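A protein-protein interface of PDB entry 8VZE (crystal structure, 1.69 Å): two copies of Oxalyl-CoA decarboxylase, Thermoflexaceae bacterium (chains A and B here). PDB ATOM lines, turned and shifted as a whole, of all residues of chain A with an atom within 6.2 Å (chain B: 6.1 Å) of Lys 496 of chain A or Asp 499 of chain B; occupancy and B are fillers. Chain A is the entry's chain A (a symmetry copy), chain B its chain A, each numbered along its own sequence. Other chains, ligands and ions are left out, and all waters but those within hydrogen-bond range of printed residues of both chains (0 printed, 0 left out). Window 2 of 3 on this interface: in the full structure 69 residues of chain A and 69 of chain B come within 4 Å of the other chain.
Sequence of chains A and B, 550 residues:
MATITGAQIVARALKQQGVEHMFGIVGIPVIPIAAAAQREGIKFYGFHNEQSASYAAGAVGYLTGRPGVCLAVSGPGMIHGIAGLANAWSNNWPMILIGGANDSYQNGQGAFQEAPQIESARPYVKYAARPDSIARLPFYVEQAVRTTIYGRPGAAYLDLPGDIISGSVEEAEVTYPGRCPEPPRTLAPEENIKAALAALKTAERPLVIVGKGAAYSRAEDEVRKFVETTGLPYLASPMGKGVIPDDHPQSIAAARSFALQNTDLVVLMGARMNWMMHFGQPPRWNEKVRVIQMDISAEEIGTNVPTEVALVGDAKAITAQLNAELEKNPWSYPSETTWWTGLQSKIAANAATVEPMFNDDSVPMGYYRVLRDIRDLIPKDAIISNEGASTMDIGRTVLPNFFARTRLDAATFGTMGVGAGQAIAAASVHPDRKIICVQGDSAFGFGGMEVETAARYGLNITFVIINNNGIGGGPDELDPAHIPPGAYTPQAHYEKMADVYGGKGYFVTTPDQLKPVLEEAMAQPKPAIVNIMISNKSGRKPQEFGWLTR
N of His 493 of chain B is in hydrogen-bond range of O of Val 500 of chain A, 2.9 Å away. The backbone carbonyl oxygen of Val 500 of chain B is in hydrogen-bond range of the backbone NH of His 493 of chain A (2.9 Å).
ND1 of His 493 of chain B lies within hydrogen-bond range of OE2 of Glu 495 of chain B. A ring nitrogen (ND1) of His 493 of chain A is in hydrogen-bond range of the side-chain carboxylate (OE2) of Glu 495 of chain A.
Among the printed residues, pairs that only touch across the chains: Ala 492 of chain A with Val 500 of chain B, Lys 496 of chain A with Asp 499 of chain B, Asp 499 of chain A with Lys 496 of chain B, Asp 499 of chain A with His 493 of chain B, His 493 of chain A with Asp 499 of chain B, Met 497 of chain A with Met 497 of chain B, Lys 496 of chain A with Lys 496 of chain B and Tyr 494 of chain A with Val 500 of chain B.
Of the printed residues of chain B, His 493 of chain A touches Asp 499 (3.7 Å) and Val 500 (2.9 Å). Lys 496 of chain A touches two residues of chain B. Ile 529 of chain A touches none of the printed residues of chain B. Of the printed residues of chain A, His 493 of chain B touches Asp 499 and Val 500. Glu 495 of chain B touches none of the printed residues of chain A. Asp 499 of chain B touches two residues of chain A. Printed residues of chain A within 4 Å of Val 500 of chain B: Ala 492, His 493 and Tyr 494. The nearest residue of chain B that does not touch Lys 496 of chain A is Val 500 of chain B (4.6 Å). The nearest residue of chain A that does not touch Asp 499 of chain B is Asp 499 of chain A (5.2 Å). The nearest printed residue of chain B that does not touch Ala 492 of chain A is Tyr 501 of chain B (5.6 Å).
Printed residues of chain B that touch a printed residue of chain A: His 493, Lys 496, Met 497, Asp 499 and Val 500. Hydrophobic or aromatic side chains of chain B that line the printed part of chain A: His 493, Met 497 and Val 500. Printed residues of chain A that touch a printed residue of chain B: Ala 492, His 493, Tyr 494, Lys 496, Met 497, Asp 499 and Val 500. Hydrophobic or aromatic side chains of chain A within 4 Å of the printed part of chain B: Ala 492, His 493, Tyr 494, Met 497 and Val 500. Among the printed residues, 10 pairs touch across the chains.
His 493 of chain A touches Asp 499 of chain B, and with the chains exchanged Asp 499 of chain A touches His 493 of chain B. His 493 of chain A touches Val 500 of chain B, and with the chains exchanged Val 500 of chain A touches His 493 of chain B. Lys 496 of chain A touches Asp 499 of chain B, and with the chains exchanged Asp 499 of chain A touches Lys 496 of chain B. Met 497 of chain B touches its own counterpart, Met 497 of chain A. 8 positions are printed for both chains. Of the 10 pairs that touch across the chains among the printed residues, 8 have their exchanged pair printed and touching as well.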
ATOM      1  N   ALA A 492      -5.748 -30.915   0.373  1.00  0.00           N
ATOM      2  CA  ALA A 492      -6.397 -29.609   0.233  1.00  0.00           C
ATOM      3  C   ALA A 492      -7.903 -29.771   0.332  1.00  0.00           C
ATOM      4  O   ALA A 492      -8.485 -30.628  -0.337  1.00  0.00           O
ATOM      5  CB  ALA A 492      -6.040 -28.983  -1.102  1.00  0.00           C
ATOM      6  N   HIS A 493      -8.542 -28.965   1.179  1.00  0.00           N
ATOM      7  CA  HIS A 493      -9.972 -29.152   1.450  1.00  0.00           C
ATOM      8  C   HIS A 493     -10.832 -28.317   0.498  1.00  0.00           C
ATOM      9  O   HIS A 493     -11.557 -27.393   0.896  1.00  0.00           O
ATOM     10  CB  HIS A 493     -10.278 -28.828   2.908  1.00  0.00           C
ATOM     11  CG  HIS A 493      -9.867 -29.926   3.829  1.00  0.00           C
ATOM     12  ND1 HIS A 493     -10.696 -30.981   4.142  1.00  0.00           N
ATOM     13  CD2 HIS A 493      -8.686 -30.183   4.434  1.00  0.00           C
ATOM     14  CE1 HIS A 493     -10.052 -31.827   4.930  1.00  0.00           C
ATOM     15  NE2 HIS A 493      -8.831 -31.365   5.127  1.00  0.00           N
ATOM     16  N   TYR A 494     -10.781 -28.691  -0.781  1.00  0.00           N
ATOM     17  CA  TYR A 494     -11.551 -27.948  -1.787  1.00  0.00           C
ATOM     18  C   TYR A 494     -13.050 -27.953  -1.488  1.00  0.00           C
ATOM     19  O   TYR A 494     -13.776 -27.048  -1.941  1.00  0.00           O
ATOM     20  CB  TYR A 494     -11.343 -28.549  -3.182  1.00  0.00           C
ATOM     21  CG  TYR A 494      -9.917 -28.472  -3.651  1.00  0.00           C
ATOM     22  CD1 TYR A 494      -9.324 -27.244  -3.901  1.00  0.00           C
ATOM     23  CD2 TYR A 494      -9.171 -29.632  -3.847  1.00  0.00           C
ATOM     24  CE1 TYR A 494      -7.994 -27.153  -4.305  1.00  0.00           C
ATOM     25  CE2 TYR A 494      -7.863 -29.561  -4.289  1.00  0.00           C
ATOM     26  CZ  TYR A 494      -7.278 -28.320  -4.511  1.00  0.00           C
ATOM     27  OH  TYR A 494      -5.972 -28.254  -4.936  1.00  0.00           O
ATOM     28  N   GLU A 495     -13.537 -28.953  -0.758  1.00  0.00           N
ATOM     29  CA  GLU A 495     -14.966 -29.020  -0.495  1.00  0.00           C
ATOM     30  C   GLU A 495     -15.414 -27.876   0.410  1.00  0.00           C
ATOM     31  O   GLU A 495     -16.614 -27.564   0.449  1.00  0.00           O
ATOM     32  CB  GLU A 495     -15.326 -30.385   0.108  1.00  0.00           C
ATOM     33  CG  GLU A 495     -15.012 -30.518   1.648  1.00  0.00           C
ATOM     34  CD  GLU A 495     -13.527 -30.707   1.993  1.00  0.00           C
ATOM     35  OE1 GLU A 495     -12.673 -30.806   1.071  1.00  0.00           O
ATOM     36  OE2 GLU A 495     -13.241 -30.767   3.228  1.00  0.00           O
ATOM     37  N   LYS A 496     -14.472 -27.192   1.100  1.00  0.00           N
ATOM     38  CA  LYS A 496     -14.867 -26.013   1.860  1.00  0.00           C
ATOM     39  C   LYS A 496     -15.331 -24.889   0.950  1.00  0.00           C
ATOM     40  O   LYS A 496     -16.016 -23.972   1.421  1.00  0.00           O
ATOM     41  CB  LYS A 496     -13.730 -25.504   2.751  1.00  0.00           C
ATOM     42  CG  LYS A 496     -13.229 -26.522   3.748  1.00  0.00           C
ATOM     43  CD  LYS A 496     -14.289 -26.865   4.767  1.00  0.00           C
ATOM     44  CE  LYS A 496     -13.658 -27.460   6.020  1.00  0.00           C
ATOM     45  NZ  LYS A 496     -14.671 -28.169   6.844  1.00  0.00           N
ATOM     46  N   MET A 497     -14.986 -24.925  -0.341  1.00  0.00           N
ATOM     47  CA  MET A 497     -15.543 -23.938  -1.252  1.00  0.00           C
ATOM     48  C   MET A 497     -17.065 -24.010  -1.325  1.00  0.00           C
ATOM     49  O   MET A 497     -17.697 -23.014  -1.673  1.00  0.00           O
ATOM     50  CB  MET A 497     -14.909 -24.108  -2.621  1.00  0.00           C
ATOM     51  CG  MET A 497     -13.423 -23.753  -2.524  1.00  0.00           C
ATOM     52  SD  MET A 497     -12.641 -23.752  -4.124  1.00  0.00           S
ATOM     53  CE  MET A 497     -13.497 -22.350  -4.903  1.00  0.00           C
ATOM     54  N   ALA A 498     -17.671 -25.139  -0.971  1.00  0.00           N
ATOM     55  CA  ALA A 498     -19.135 -25.160  -0.971  1.00  0.00           C
ATOM     56  C   ALA A 498     -19.696 -24.223   0.092  1.00  0.00           C
ATOM     57  O   ALA A 498     -20.788 -23.677  -0.077  1.00  0.00           O
ATOM     58  CB  ALA A 498     -19.630 -26.613  -0.797  1.00  0.00           C
ATOM     59  N   ASP A 499     -18.936 -23.947   1.157  1.00  0.00           N
ATOM     60  CA  ASP A 499     -19.396 -23.001   2.166  1.00  0.00           C
ATOM     61  C   ASP A 499     -19.447 -21.565   1.668  1.00  0.00           C
ATOM     62  O   ASP A 499     -20.053 -20.718   2.342  1.00  0.00           O
ATOM     63  CB  ASP A 499     -18.492 -23.060   3.404  1.00  0.00           C
ATOM     64  CG  ASP A 499     -18.518 -24.415   4.088  1.00  0.00           C
ATOM     65  OD1 ASP A 499     -19.535 -25.124   3.978  1.00  0.00           O
ATOM     66  OD2 ASP A 499     -17.521 -24.772   4.748  1.00  0.00           O
ATOM     67  N   VAL A 500     -18.830 -21.264   0.520  1.00  0.00           N
ATOM     68  CA  VAL A 500     -18.875 -19.903   0.003  1.00  0.00           C
ATOM     69  C   VAL A 500     -20.310 -19.507  -0.304  1.00  0.00           C
ATOM     70  O   VAL A 500     -20.735 -18.371  -0.033  1.00  0.00           O
ATOM     71  CB  VAL A 500     -17.981 -19.796  -1.241  1.00  0.00           C
ATOM     72  CG1 VAL A 500     -18.142 -18.420  -1.886  1.00  0.00           C
ATOM     73  CG2 VAL A 500     -16.524 -20.039  -0.847  1.00  0.00           C
ATOM     74  N   GLY A 505     -20.209 -29.469   1.514  1.00  0.00           N
ATOM     75  CA  GLY A 505     -18.941 -30.041   1.075  1.00  0.00           C
ATOM     76  C   GLY A 505     -18.668 -31.306   1.866  1.00  0.00           C
ATOM     77  O   GLY A 505     -18.984 -31.381   3.063  1.00  0.00           O
ATOM     78  N   ILE A 529     -19.974 -30.285  -3.249  1.00  0.00           N
ATOM     79  CA  ILE A 529     -18.609 -30.624  -3.679  1.00  0.00           C
ATOM     80  C   ILE A 529     -18.152 -31.827  -2.873  1.00  0.00           C
ATOM     81  O   ILE A 529     -18.140 -31.796  -1.628  1.00  0.00           O
ATOM     82  CB  ILE A 529     -17.620 -29.454  -3.517  1.00  0.00           C
ATOM     83  CG1 ILE A 529     -18.143 -28.210  -4.281  1.00  0.00           C
ATOM     84  CG2 ILE A 529     -16.250 -29.854  -4.045  1.00  0.00           C
ATOM     85  CD1 ILE A 529     -17.312 -26.925  -4.056  1.00  0.00           C
ATOM     86  N   HIS B 493     -19.225 -16.252   1.246  1.00  0.00           N
ATOM     87  CA  HIS B 493     -18.214 -16.425   2.296  1.00  0.00           C
ATOM     88  C   HIS B 493     -16.865 -16.840   1.705  1.00  0.00           C
ATOM     89  O   HIS B 493     -16.343 -17.938   1.948  1.00  0.00           O
ATOM     90  CB  HIS B 493     -18.701 -17.428   3.335  1.00  0.00           C
ATOM     91  CG  HIS B 493     -19.700 -16.834   4.269  1.00  0.00           C
ATOM     92  ND1 HIS B 493     -19.336 -16.179   5.425  1.00  0.00           N
ATOM     93  CD2 HIS B 493     -21.043 -16.716   4.175  1.00  0.00           C
ATOM     94  CE1 HIS B 493     -20.420 -15.709   6.023  1.00  0.00           C
ATOM     95  NE2 HIS B 493     -21.471 -16.025   5.287  1.00  0.00           N
ATOM     96  N   GLU B 495     -14.037 -16.100   2.578  1.00  0.00           N
ATOM     97  CA  GLU B 495     -13.006 -16.374   3.566  1.00  0.00           C
ATOM     98  C   GLU B 495     -12.955 -17.858   3.914  1.00  0.00           C
ATOM     99  O   GLU B 495     -11.936 -18.325   4.445  1.00  0.00           O
ATOM    100  CB  GLU B 495     -13.234 -15.512   4.816  1.00  0.00           C
ATOM    101  CG  GLU B 495     -14.345 -16.063   5.790  1.00  0.00           C
ATOM    102  CD  GLU B 495     -15.790 -15.839   5.317  1.00  0.00           C
ATOM    103  OE1 GLU B 495     -16.014 -15.201   4.255  1.00  0.00           O
ATOM    104  OE2 GLU B 495     -16.703 -16.316   6.059  1.00  0.00           O
ATOM    105  N   LYS B 496     -14.008 -18.637   3.573  1.00  0.00           N
ATOM    106  CA  LYS B 496     -13.918 -20.077   3.776  1.00  0.00           C
ATOM    107  C   LYS B 496     -12.877 -20.707   2.866  1.00  0.00           C
ATOM    108  O   LYS B 496     -12.429 -21.827   3.143  1.00  0.00           O
ATOM    109  CB  LYS B 496     -15.267 -20.768   3.551  1.00  0.00           C
ATOM    110  CG  LYS B 496     -16.370 -20.266   4.453  1.00  0.00           C
ATOM    111  CD  LYS B 496     -16.092 -20.593   5.900  1.00  0.00           C
ATOM    112  CE  LYS B 496     -17.381 -20.561   6.715  1.00  0.00           C
ATOM    113  NZ  LYS B 496     -17.090 -20.472   8.170  1.00  0.00           N
ATOM    114  N   MET B 497     -12.471 -20.027   1.789  1.00  0.00           N
ATOM    115  CA  MET B 497     -11.372 -20.550   0.992  1.00  0.00           C
ATOM    116  C   MET B 497     -10.082 -20.677   1.797  1.00  0.00           C
ATOM    117  O   MET B 497      -9.224 -21.479   1.433  1.00  0.00           O
ATOM    118  CB  MET B 497     -11.182 -19.674  -0.233  1.00  0.00           C
ATOM    119  CG  MET B 497     -12.415 -19.811  -1.133  1.00  0.00           C
ATOM    120  SD  MET B 497     -12.198 -18.956  -2.679  1.00  0.00           S
ATOM    121  CE  MET B 497     -10.862 -19.946  -3.414  1.00  0.00           C
ATOM    122  N   ALA B 498      -9.937 -19.943   2.896  1.00  0.00           N
ATOM    123  CA  ALA B 498      -8.728 -20.139   3.697  1.00  0.00           C
ATOM    124  C   ALA B 498      -8.699 -21.533   4.313  1.00  0.00           C
ATOM    125  O   ALA B 498      -7.623 -22.092   4.531  1.00  0.00           O
ATOM    126  CB  ALA B 498      -8.624 -19.022   4.759  1.00  0.00           C
ATOM    127  N   ASP B 499      -9.864 -22.156   4.523  1.00  0.00           N
ATOM    128  CA  ASP B 499      -9.888 -23.518   5.042  1.00  0.00           C
ATOM    129  C   ASP B 499      -9.366 -24.550   4.055  1.00  0.00           C
ATOM    130  O   ASP B 499      -9.104 -25.691   4.464  1.00  0.00           O
ATOM    131  CB  ASP B 499     -11.315 -23.906   5.451  1.00  0.00           C
ATOM    132  CG  ASP B 499     -11.862 -23.042   6.573  1.00  0.00           C
ATOM    133  OD1 ASP B 499     -11.064 -22.521   7.373  1.00  0.00           O
ATOM    134  OD2 ASP B 499     -13.097 -22.889   6.664  1.00  0.00           O
ATOM    135  N   VAL B 500      -9.214 -24.190   2.776  1.00  0.00           N
ATOM    136  CA  VAL B 500      -8.696 -25.147   1.806  1.00  0.00           C
ATOM    137  C   VAL B 500      -7.284 -25.562   2.183  1.00  0.00           C
ATOM    138  O   VAL B 500      -6.911 -26.743   2.076  1.00  0.00           O
ATOM    139  CB  VAL B 500      -8.750 -24.533   0.400  1.00  0.00           C
ATOM    140  CG1 VAL B 500      -8.066 -25.461  -0.603  1.00  0.00           C
ATOM    141  CG2 VAL B 500     -10.206 -24.290   0.002  1.00  0.00           C
ATOM    142  N   TYR B 501      -6.476 -24.602   2.659  1.00  0.00           N
ATOM    143  CA  TYR B 501      -5.056 -24.844   2.926  1.00  0.00           C
ATOM    144  C   TYR B 501      -4.719 -24.685   4.403  1.00  0.00           C
ATOM    145  O   TYR B 501      -3.543 -24.698   4.767  1.00  0.00           O
ATOM    146  CB  TYR B 501      -4.179 -23.904   2.075  1.00  0.00           C
ATOM    147  CG  TYR B 501      -4.551 -22.431   2.211  1.00  0.00           C
ATOM    148  CD1 TYR B 501      -4.071 -21.671   3.272  1.00  0.00           C
ATOM    149  CD2 TYR B 501      -5.399 -21.804   1.288  1.00  0.00           C
ATOM    150  CE1 TYR B 501      -4.419 -20.328   3.411  1.00  0.00           C
ATOM    151  CE2 TYR B 501      -5.742 -20.474   1.418  1.00  0.00           C
ATOM    152  CZ  TYR B 501      -5.245 -19.745   2.483  1.00  0.00           C
ATOM    153  OH  TYR B 501      -5.565 -18.423   2.622  1.00  0.00           O
ATOM    154  N   GLY B 502      -5.721 -24.585   5.269  1.00  0.00           N
ATOM    155  CA  GLY B 502      -5.450 -24.541   6.693  1.00  0.00           C
ATOM    156  C   GLY B 502      -5.109 -23.169   7.234  1.00  0.00           C
ATOM    157  O   GLY B 502      -4.505 -23.077   8.313  1.00  0.00           O
ATOM    158  N   GLY B 503      -5.474 -22.098   6.530  1.00  0.00           N
ATOM    159  CA  GLY B 503      -5.295 -20.750   7.025  1.00  0.00           C
ATOM    160  C   GLY B 503      -6.543 -20.301   7.776  1.00  0.00           C
ATOM    161  O   GLY B 503      -7.470 -21.075   8.020  1.00  0.00           O
ATOM    162  N   LYS B 504      -6.561 -19.025   8.144  1.00  0.00           N
ATOM    163  CA  LYS B 504      -7.688 -18.454   8.883  1.00  0.00           C
ATOM    164  C   LYS B 504      -8.498 -17.522   7.993  1.00  0.00           C
ATOM    165  O   LYS B 504      -7.939 -16.661   7.311  1.00  0.00           O
ATOM    166  CB  LYS B 504      -7.218 -17.694  10.126  1.00  0.00           C
ATOM    167  CG  LYS B 504      -6.548 -18.630  11.137  1.00  0.00           C
ATOM    168  CD  LYS B 504      -6.197 -17.892  12.436  1.00  0.00           C
ATOM    169  CE  LYS B 504      -5.658 -18.855  13.505  1.00  0.00           C
ATOM    170  NZ  LYS B 504      -6.703 -19.840  13.915  1.00  0.00           N
ATOM    171  N   GLY B 505      -9.813 -17.681   8.018  1.00  0.00           N
ATOM    172  CA  GLY B 505     -10.710 -16.791   7.289  1.00  0.00           C
ATOM    173  C   GLY B 505     -11.550 -16.012   8.283  1.00  0.00           C
ATOM    174  O   GLY B 505     -11.945 -16.547   9.329  1.00  0.00           O
